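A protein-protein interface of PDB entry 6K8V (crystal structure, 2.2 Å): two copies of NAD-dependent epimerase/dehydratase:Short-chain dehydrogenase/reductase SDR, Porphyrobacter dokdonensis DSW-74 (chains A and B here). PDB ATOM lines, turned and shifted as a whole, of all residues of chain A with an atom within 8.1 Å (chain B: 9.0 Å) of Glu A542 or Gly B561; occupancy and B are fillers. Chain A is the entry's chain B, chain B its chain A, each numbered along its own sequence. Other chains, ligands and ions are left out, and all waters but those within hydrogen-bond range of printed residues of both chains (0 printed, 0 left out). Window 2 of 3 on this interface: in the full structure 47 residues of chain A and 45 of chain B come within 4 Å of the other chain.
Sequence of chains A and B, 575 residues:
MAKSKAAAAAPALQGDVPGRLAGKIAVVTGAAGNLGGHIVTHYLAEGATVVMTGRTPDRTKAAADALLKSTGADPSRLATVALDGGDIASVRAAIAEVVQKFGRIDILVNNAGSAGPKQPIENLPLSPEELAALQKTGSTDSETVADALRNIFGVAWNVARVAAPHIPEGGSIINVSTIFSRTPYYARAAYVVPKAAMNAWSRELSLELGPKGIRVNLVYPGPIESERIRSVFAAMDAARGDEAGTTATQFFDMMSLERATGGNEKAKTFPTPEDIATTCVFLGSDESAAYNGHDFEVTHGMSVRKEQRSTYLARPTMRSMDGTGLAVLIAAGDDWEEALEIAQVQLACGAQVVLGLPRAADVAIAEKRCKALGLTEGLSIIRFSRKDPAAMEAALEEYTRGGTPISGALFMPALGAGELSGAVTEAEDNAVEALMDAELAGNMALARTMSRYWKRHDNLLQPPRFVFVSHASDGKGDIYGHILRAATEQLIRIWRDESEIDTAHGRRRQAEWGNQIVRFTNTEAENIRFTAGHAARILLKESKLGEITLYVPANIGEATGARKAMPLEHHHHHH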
ATOM      1  N   ARG A 319     -23.935  12.378  -9.186  1.00  0.00           N
ATOM      2  CA  ARG A 319     -22.875  13.333  -9.617  1.00  0.00           C
ATOM      3  C   ARG A 319     -23.180  13.775 -11.054  1.00  0.00           C
ATOM      4  O   ARG A 319     -24.033  13.128 -11.698  1.00  0.00           O
ATOM      5  CB  ARG A 319     -21.482  12.708  -9.471  1.00  0.00           C
ATOM      6  CG  ARG A 319     -21.058  12.452  -8.030  1.00  0.00           C
ATOM      7  CD  ARG A 319     -21.541  11.115  -7.491  1.00  0.00           C
ATOM      8  NE  ARG A 319     -20.882   9.984  -8.145  1.00  0.00           N
ATOM      9  CZ  ARG A 319     -20.246   8.983  -7.529  1.00  0.00           C
ATOM     10  NH1 ARG A 319     -20.182   8.928  -6.209  1.00  0.00           N
ATOM     11  NH2 ARG A 319     -19.680   8.022  -8.242  1.00  0.00           N
ATOM     12  N   ASP A 322     -21.530  11.296 -13.867  1.00  0.00           N
ATOM     13  CA  ASP A 322     -22.030   9.895 -13.832  1.00  0.00           C
ATOM     14  C   ASP A 322     -22.317   9.378 -15.254  1.00  0.00           C
ATOM     15  O   ASP A 322     -22.038   8.189 -15.502  1.00  0.00           O
ATOM     16  CB  ASP A 322     -23.294   9.777 -12.969  1.00  0.00           C
ATOM     17  CG  ASP A 322     -23.082   9.634 -11.466  1.00  0.00           C
ATOM     18  OD1 ASP A 322     -21.937   9.365 -11.052  1.00  0.00           O
ATOM     19  OD2 ASP A 322     -24.088   9.769 -10.713  1.00  0.00           O
ATOM     20  N   LEU A 326     -22.781   7.678 -21.908  1.00  0.00           N
ATOM     21  CA  LEU A 326     -24.035   6.876 -21.858  1.00  0.00           C
ATOM     22  C   LEU A 326     -25.188   7.659 -22.481  1.00  0.00           C
ATOM     23  O   LEU A 326     -25.214   8.943 -22.370  1.00  0.00           O
ATOM     24  CB  LEU A 326     -24.355   6.527 -20.411  1.00  0.00           C
ATOM     25  CG  LEU A 326     -23.184   5.930 -19.636  1.00  0.00           C
ATOM     26  CD1 LEU A 326     -23.504   5.836 -18.148  1.00  0.00           C
ATOM     27  CD2 LEU A 326     -22.798   4.576 -20.213  1.00  0.00           C
ATOM     28  N   LEU A 461     -20.338   0.700 -22.945  1.00  0.00           N
ATOM     29  CA  LEU A 461     -19.375   1.134 -21.902  1.00  0.00           C
ATOM     30  C   LEU A 461     -19.713   0.422 -20.589  1.00  0.00           C
ATOM     31  O   LEU A 461     -18.782  -0.011 -19.924  1.00  0.00           O
ATOM     32  CB  LEU A 461     -19.480   2.651 -21.741  1.00  0.00           C
ATOM     33  CG  LEU A 461     -18.778   3.472 -22.817  1.00  0.00           C
ATOM     34  CD1 LEU A 461     -18.941   4.956 -22.569  1.00  0.00           C
ATOM     35  CD2 LEU A 461     -17.309   3.106 -22.901  1.00  0.00           C
ATOM     36  N   GLN A 462     -21.004   0.305 -20.268  1.00  0.00           N
ATOM     37  CA  GLN A 462     -21.526  -0.416 -19.084  1.00  0.00           C
ATOM     38  C   GLN A 462     -22.543  -1.454 -19.574  1.00  0.00           C
ATOM     39  O   GLN A 462     -23.198  -1.193 -20.579  1.00  0.00           O
ATOM     40  CB  GLN A 462     -22.237   0.585 -18.184  1.00  0.00           C
ATOM     41  CG  GLN A 462     -21.297   1.486 -17.415  1.00  0.00           C
ATOM     42  CD  GLN A 462     -22.082   2.545 -16.689  1.00  0.00           C
ATOM     43  OE1 GLN A 462     -23.301   2.482 -16.602  1.00  0.00           O
ATOM     44  NE2 GLN A 462     -21.376   3.534 -16.174  1.00  0.00           N
ATOM     45  N   PRO A 463     -22.701  -2.629 -18.934  1.00  0.00           N
ATOM     46  CA  PRO A 463     -23.705  -3.598 -19.383  1.00  0.00           C
ATOM     47  C   PRO A 463     -25.065  -2.915 -19.334  1.00  0.00           C
ATOM     48  O   PRO A 463     -25.272  -2.038 -18.505  1.00  0.00           O
ATOM     49  CB  PRO A 463     -23.581  -4.791 -18.438  1.00  0.00           C
ATOM     50  CG  PRO A 463     -22.735  -4.275 -17.263  1.00  0.00           C
ATOM     51  CD  PRO A 463     -21.926  -3.100 -17.776  1.00  0.00           C
ATOM     52  N   ARG A 465     -29.029  -1.612 -19.015  1.00  0.00           N
ATOM     53  CA  ARG A 465     -29.926  -1.426 -17.850  1.00  0.00           C
ATOM     54  C   ARG A 465     -31.248  -0.839 -18.358  1.00  0.00           C
ATOM     55  O   ARG A 465     -31.187   0.053 -19.188  1.00  0.00           O
ATOM     56  CB  ARG A 465     -29.237  -0.539 -16.809  1.00  0.00           C
ATOM     57  CG  ARG A 465     -28.008  -1.174 -16.171  1.00  0.00           C
ATOM     58  CD  ARG A 465     -28.411  -2.189 -15.110  1.00  0.00           C
ATOM     59  NE  ARG A 465     -27.288  -2.820 -14.423  1.00  0.00           N
ATOM     60  CZ  ARG A 465     -26.527  -3.789 -14.940  1.00  0.00           C
ATOM     61  NH1 ARG A 465     -26.749  -4.251 -16.162  1.00  0.00           N
ATOM     62  NH2 ARG A 465     -25.556  -4.310 -14.218  1.00  0.00           N
ATOM     63  N   ALA A 536     -32.052   7.388 -12.594  1.00  0.00           N
ATOM     64  CA  ALA A 536     -30.683   7.780 -12.994  1.00  0.00           C
ATOM     65  C   ALA A 536     -29.666   6.827 -12.347  1.00  0.00           C
ATOM     66  O   ALA A 536     -28.717   6.426 -13.056  1.00  0.00           O
ATOM     67  CB  ALA A 536     -30.421   9.224 -12.634  1.00  0.00           C
ATOM     68  N   ARG A 537     -29.854   6.438 -11.076  1.00  0.00           N
ATOM     69  CA  ARG A 537     -28.870   5.594 -10.338  1.00  0.00           C
ATOM     70  C   ARG A 537     -28.843   4.197 -10.947  1.00  0.00           C
ATOM     71  O   ARG A 537     -27.751   3.590 -11.028  1.00  0.00           O
ATOM     72  CB  ARG A 537     -29.198   5.462  -8.851  1.00  0.00           C
ATOM     73  CG  ARG A 537     -29.412   6.783  -8.123  1.00  0.00           C
ATOM     74  CD  ARG A 537     -29.388   6.662  -6.604  1.00  0.00           C
ATOM     75  NE  ARG A 537     -28.031   6.897  -6.149  1.00  0.00           N
ATOM     76  CZ  ARG A 537     -27.210   5.980  -5.655  1.00  0.00           C
ATOM     77  NH1 ARG A 537     -27.614   4.732  -5.482  1.00  0.00           N
ATOM     78  NH2 ARG A 537     -25.985   6.332  -5.308  1.00  0.00           N
ATOM     79  N   ILE A 538     -30.008   3.674 -11.306  1.00  0.00           N
ATOM     80  CA  ILE A 538     -30.099   2.325 -11.923  1.00  0.00           C
ATOM     81  C   ILE A 538     -29.491   2.403 -13.322  1.00  0.00           C
ATOM     82  O   ILE A 538     -28.804   1.448 -13.725  1.00  0.00           O
ATOM     83  CB  ILE A 538     -31.546   1.789 -11.907  1.00  0.00           C
ATOM     84  CG1 ILE A 538     -31.947   1.388 -10.486  1.00  0.00           C
ATOM     85  CG2 ILE A 538     -31.703   0.608 -12.841  1.00  0.00           C
ATOM     86  CD1 ILE A 538     -33.408   1.550 -10.173  1.00  0.00           C
ATOM     87  N   LEU A 539     -29.713   3.498 -14.058  1.00  0.00           N
ATOM     88  CA  LEU A 539     -29.311   3.571 -15.498  1.00  0.00           C
ATOM     89  C   LEU A 539     -27.842   3.989 -15.668  1.00  0.00           C
ATOM     90  O   LEU A 539     -27.204   3.457 -16.598  1.00  0.00           O
ATOM     91  CB  LEU A 539     -30.239   4.530 -16.236  1.00  0.00           C
ATOM     92  CG  LEU A 539     -31.688   4.077 -16.329  1.00  0.00           C
ATOM     93  CD1 LEU A 539     -32.494   5.144 -17.042  1.00  0.00           C
ATOM     94  CD2 LEU A 539     -31.812   2.728 -17.028  1.00  0.00           C
ATOM     95  N   LEU A 540     -27.317   4.876 -14.826  1.00  0.00           N
ATOM     96  CA  LEU A 540     -26.025   5.550 -15.121  1.00  0.00           C
ATOM     97  C   LEU A 540     -24.906   5.040 -14.209  1.00  0.00           C
ATOM     98  O   LEU A 540     -23.799   4.858 -14.751  1.00  0.00           O
ATOM     99  CB  LEU A 540     -26.214   7.062 -15.002  1.00  0.00           C
ATOM    100  CG  LEU A 540     -27.322   7.633 -15.878  1.00  0.00           C
ATOM    101  CD1 LEU A 540     -27.546   9.103 -15.571  1.00  0.00           C
ATOM    102  CD2 LEU A 540     -27.021   7.406 -17.352  1.00  0.00           C
ATOM    103  N   LYS A 541     -25.168   4.804 -12.910  1.00  0.00           N
ATOM    104  CA  LYS A 541     -24.193   4.152 -11.981  1.00  0.00           C
ATOM    105  C   LYS A 541     -24.001   2.675 -12.362  1.00  0.00           C
ATOM    106  O   LYS A 541     -24.914   2.082 -12.980  1.00  0.00           O
ATOM    107  CB  LYS A 541     -24.624   4.289 -10.515  1.00  0.00           C
ATOM    108  CG  LYS A 541     -24.480   5.689  -9.936  1.00  0.00           C
ATOM    109  CD  LYS A 541     -24.288   5.721  -8.428  1.00  0.00           C
ATOM    110  CE  LYS A 541     -23.135   6.609  -7.992  1.00  0.00           C
ATOM    111  NZ  LYS A 541     -22.559   6.181  -6.692  1.00  0.00           N
ATOM    112  N   GLU A 542     -22.830   2.118 -12.035  1.00  0.00           N
ATOM    113  CA  GLU A 542     -22.504   0.673 -12.191  1.00  0.00           C
ATOM    114  C   GLU A 542     -23.011  -0.059 -10.947  1.00  0.00           C
ATOM    115  O   GLU A 542     -22.366   0.060  -9.883  1.00  0.00           O
ATOM    116  CB  GLU A 542     -21.001   0.430 -12.315  1.00  0.00           C
ATOM    117  CG  GLU A 542     -20.342   1.141 -13.479  1.00  0.00           C
ATOM    118  CD  GLU A 542     -19.100   0.402 -13.944  1.00  0.00           C
ATOM    119  OE1 GLU A 542     -17.982   0.777 -13.494  1.00  0.00           O
ATOM    120  OE2 GLU A 542     -19.267  -0.582 -14.708  1.00  0.00           O
ATOM    121  N   SER A 543     -24.133  -0.765 -11.082  1.00  0.00           N
ATOM    122  CA  SER A 543     -24.903  -1.371  -9.968  1.00  0.00           C
ATOM    123  C   SER A 543     -25.772  -2.505 -10.504  1.00  0.00           C
ATOM    124  O   SER A 543     -26.019  -2.560 -11.729  1.00  0.00           O
ATOM    125  CB  SER A 543     -25.739  -0.344  -9.243  1.00  0.00           C
ATOM    126  OG  SER A 543     -26.594   0.336 -10.146  1.00  0.00           O
ATOM    127  N   LYS A 544     -26.119  -3.413  -9.597  1.00  0.00           N
ATOM    128  CA  LYS A 544     -27.084  -4.527  -9.772  1.00  0.00           C
ATOM    129  C   LYS A 544     -27.967  -4.497  -8.520  1.00  0.00           C
ATOM    130  O   LYS A 544     -27.430  -4.729  -7.422  1.00  0.00           O
ATOM    131  CB  LYS A 544     -26.319  -5.836  -9.970  1.00  0.00           C
ATOM    132  CG  LYS A 544     -26.977  -6.852 -10.887  1.00  0.00           C
ATOM    133  CD  LYS A 544     -26.050  -7.999 -11.227  1.00  0.00           C
ATOM    134  CE  LYS A 544     -26.416  -8.705 -12.519  1.00  0.00           C
ATOM    135  NZ  LYS A 544     -25.224  -9.057 -13.327  1.00  0.00           N
ATOM    136  N   LEU A 545     -29.210  -4.043  -8.652  1.00  0.00           N
ATOM    137  CA  LEU A 545     -30.199  -3.989  -7.544  1.00  0.00           C
ATOM    138  C   LEU A 545     -30.910  -5.335  -7.555  1.00  0.00           C
ATOM    139  O   LEU A 545     -31.687  -5.544  -8.510  1.00  0.00           O
ATOM    140  CB  LEU A 545     -31.212  -2.862  -7.768  1.00  0.00           C
ATOM    141  CG  LEU A 545     -30.793  -1.465  -7.332  1.00  0.00           C
ATOM    142  CD1 LEU A 545     -31.070  -1.269  -5.868  1.00  0.00           C
ATOM    143  CD2 LEU A 545     -29.333  -1.191  -7.649  1.00  0.00           C
ATOM    144  N   LEU B 313     -30.741  -0.123   0.162  1.00  0.00           N
ATOM    145  CA  LEU B 313     -30.153   0.209  -1.179  1.00  0.00           C
ATOM    146  C   LEU B 313     -29.168   1.386  -1.081  1.00  0.00           C
ATOM    147  O   LEU B 313     -28.913   2.020  -2.137  1.00  0.00           O
ATOM    148  CB  LEU B 313     -31.254   0.577  -2.185  1.00  0.00           C
ATOM    149  CG  LEU B 313     -32.341  -0.468  -2.385  1.00  0.00           C
ATOM    150  CD1 LEU B 313     -33.226  -0.070  -3.554  1.00  0.00           C
ATOM    151  CD2 LEU B 313     -31.745  -1.859  -2.578  1.00  0.00           C
ATOM    152  N   ALA B 314     -28.621   1.670   0.105  1.00  0.00           N
ATOM    153  CA  ALA B 314     -27.759   2.852   0.334  1.00  0.00           C
ATOM    154  C   ALA B 314     -26.718   2.534   1.405  1.00  0.00           C
ATOM    155  O   ALA B 314     -27.063   1.878   2.378  1.00  0.00           O
ATOM    156  CB  ALA B 314     -28.605   4.045   0.714  1.00  0.00           C
ATOM    157  N   ARG B 315     -25.473   2.953   1.187  1.00  0.00           N
ATOM    158  CA  ARG B 315     -24.452   3.028   2.254  1.00  0.00           C
ATOM    159  C   ARG B 315     -24.973   4.043   3.257  1.00  0.00           C
ATOM    160  O   ARG B 315     -25.657   4.989   2.877  1.00  0.00           O
ATOM    161  CB  ARG B 315     -23.080   3.435   1.705  1.00  0.00           C
ATOM    162  CG  ARG B 315     -22.440   2.378   0.818  1.00  0.00           C
ATOM    163  CD  ARG B 315     -20.947   2.231   1.030  1.00  0.00           C
ATOM    164  NE  ARG B 315     -20.474   0.975   0.468  1.00  0.00           N
ATOM    165  CZ  ARG B 315     -19.271   0.773  -0.058  1.00  0.00           C
ATOM    166  NH1 ARG B 315     -18.379   1.755  -0.111  1.00  0.00           N
ATOM    167  NH2 ARG B 315     -18.966  -0.417  -0.546  1.00  0.00           N
ATOM    168  N   ASN B 555     -24.751  -8.324  -1.358  1.00  0.00           N
ATOM    169  CA  ASN B 555     -23.609  -7.604  -1.961  1.00  0.00           C
ATOM    170  C   ASN B 555     -23.794  -6.107  -1.705  1.00  0.00           C
ATOM    171  O   ASN B 555     -24.589  -5.498  -2.422  1.00  0.00           O
ATOM    172  CB  ASN B 555     -23.557  -7.913  -3.460  1.00  0.00           C
ATOM    173  CG  ASN B 555     -22.244  -7.578  -4.123  1.00  0.00           C
ATOM    174  OD1 ASN B 555     -21.839  -6.426  -4.148  1.00  0.00           O
ATOM    175  ND2 ASN B 555     -21.596  -8.574  -4.695  1.00  0.00           N
ATOM    176  N   ILE B 556     -23.081  -5.553  -0.721  1.00  0.00           N
ATOM    177  CA  ILE B 556     -23.116  -4.082  -0.438  1.00  0.00           C
ATOM    178  C   ILE B 556     -22.703  -3.271  -1.676  1.00  0.00           C
ATOM    179  O   ILE B 556     -23.368  -2.241  -1.961  1.00  0.00           O
ATOM    180  CB  ILE B 556     -22.215  -3.695   0.741  1.00  0.00           C
ATOM    181  CG1 ILE B 556     -22.750  -4.238   2.070  1.00  0.00           C
ATOM    182  CG2 ILE B 556     -22.063  -2.189   0.766  1.00  0.00           C
ATOM    183  CD1 ILE B 556     -21.707  -4.304   3.159  1.00  0.00           C
ATOM    184  N   GLY B 557     -21.597  -3.672  -2.321  1.00  0.00           N
ATOM    185  CA  GLY B 557     -20.931  -2.939  -3.418  1.00  0.00           C
ATOM    186  C   GLY B 557     -21.763  -2.903  -4.691  1.00  0.00           C
ATOM    187  O   GLY B 557     -21.505  -2.022  -5.517  1.00  0.00           O
ATOM    188  N   GLU B 558     -22.723  -3.822  -4.845  1.00  0.00           N
ATOM    189  CA  GLU B 558     -23.599  -3.944  -6.043  1.00  0.00           C
ATOM    190  C   GLU B 558     -24.923  -3.208  -5.790  1.00  0.00           C
ATOM    191  O   GLU B 558     -25.356  -2.461  -6.696  1.00  0.00           O
ATOM    192  CB  GLU B 558     -23.858  -5.416  -6.388  1.00  0.00           C
ATOM    193  CG  GLU B 558     -22.781  -6.047  -7.257  1.00  0.00           C
ATOM    194  CD  GLU B 558     -23.163  -7.342  -7.967  1.00  0.00           C
ATOM    195  OE1 GLU B 558     -24.188  -7.975  -7.588  1.00  0.00           O
ATOM    196  OE2 GLU B 558     -22.420  -7.727  -8.900  1.00  0.00           O
ATOM    197  N   ALA B 559     -25.555  -3.433  -4.627  1.00  0.00           N
ATOM    198  CA  ALA B 559     -26.839  -2.803  -4.230  1.00  0.00           C
ATOM    199  C   ALA B 559     -26.638  -1.281  -4.129  1.00  0.00           C
ATOM    200  O   ALA B 559     -27.625  -0.557  -4.365  1.00  0.00           O
ATOM    201  CB  ALA B 559     -27.372  -3.411  -2.951  1.00  0.00           C
ATOM    202  N   THR B 560     -25.408  -0.821  -3.836  1.00  0.00           N
ATOM    203  CA  THR B 560     -24.985   0.612  -3.838  1.00  0.00           C
ATOM    204  C   THR B 560     -23.701   0.766  -4.665  1.00  0.00           C
ATOM    205  O   THR B 560     -22.724   0.055  -4.350  1.00  0.00           O
ATOM    206  CB  THR B 560     -24.748   1.147  -2.419  1.00  0.00           C
ATOM    207  OG1 THR B 560     -23.384   0.937  -2.049  1.00  0.00           O
ATOM    208  CG2 THR B 560     -25.640   0.489  -1.391  1.00  0.00           C
ATOM    209  N   GLY B 561     -23.699   1.695  -5.634  1.00  0.00           N
ATOM    210  CA  GLY B 561     -22.630   1.939  -6.629  1.00  0.00           C
ATOM    211  C   GLY B 561     -21.208   1.836  -6.077  1.00  0.00           C
ATOM    212  O   GLY B 561     -20.330   1.396  -6.847  1.00  0.00           O
ATOM    213  N   ALA B 562     -20.971   2.248  -4.821  1.00  0.00           N
ATOM    214  CA  ALA B 562     -19.658   2.187  -4.130  1.00  0.00           C
ATOM    215  C   ALA B 562     -19.423   0.761  -3.624  1.00  0.00           C
ATOM    216  O   ALA B 562     -18.451   0.127  -4.029  1.00  0.00           O
ATOM    217  CB  ALA B 562     -19.590   3.187  -2.999  1.00  0.00           C
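The backbone carbonyl oxygen (O) of Glu B558 lies within hydrogen-bond range of the backbone NH (N) of Lys A544 (3.1 Å).
The side-chain amide oxygen (OD1) of Asn B555 lies within hydrogen-bond range of the backbone NH (N) of Glu B558 (2.8 Å).
O of Ser A543 lies within hydrogen-bond range of NE of Arg A465 (3.0 Å).
CA of Gly B561 touches O of Glu A542, at 3.8 Å.
CB of Ser A543 touches O of Glu B558, at 3.3 Å.
Ala B559 touches Lys A544.
Leu A545 touches Leu B313.
O of Ala B559 touches CD2 of Leu A545, at 3.8 Å.
No residue of chain B comes within 4 Å of Lys A541.
Of the printed residues of chain B, Ser A543 touches Glu B558.
Printed residues of chain B within 4 Å of Lys A544: Glu B558 (3.1 Å) and Ala B559 (3.6 Å).
Printed residues of chain A within 4 Å of Leu B313: Leu A545 (3.4 Å).
Of the printed residues of chain A, Glu B558 touches Ser A543 (3.3 Å) and Lys A544 (3.1 Å).
Thr B560 touches none of the printed residues of chain A.
Gly B561 touches just one residue of chain A: Glu A542.
The nearest residue of chain B that does not touch Glu A542 is Gly B557 (4.9 Å).
The nearest residue of chain A that does not touch Gly B561 is Lys A541 (4.2 Å).
Printed residues of chain A that touch a printed residue of chain B: Glu A542, Ser A543, Lys A544 and Leu A545.
Hydrophobic or aromatic side chains of chain A that line the printed part of chain B: Leu A545.
Among the printed residues, no Asp or Glu carboxylate lies within 4 Å of a Lys or Arg side-chain nitrogen of the other chain.
No position is printed for both chains.
Of the 6 pairs that touch across the chains among the printed residues, none has its exchanged pair printed and touching as well.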
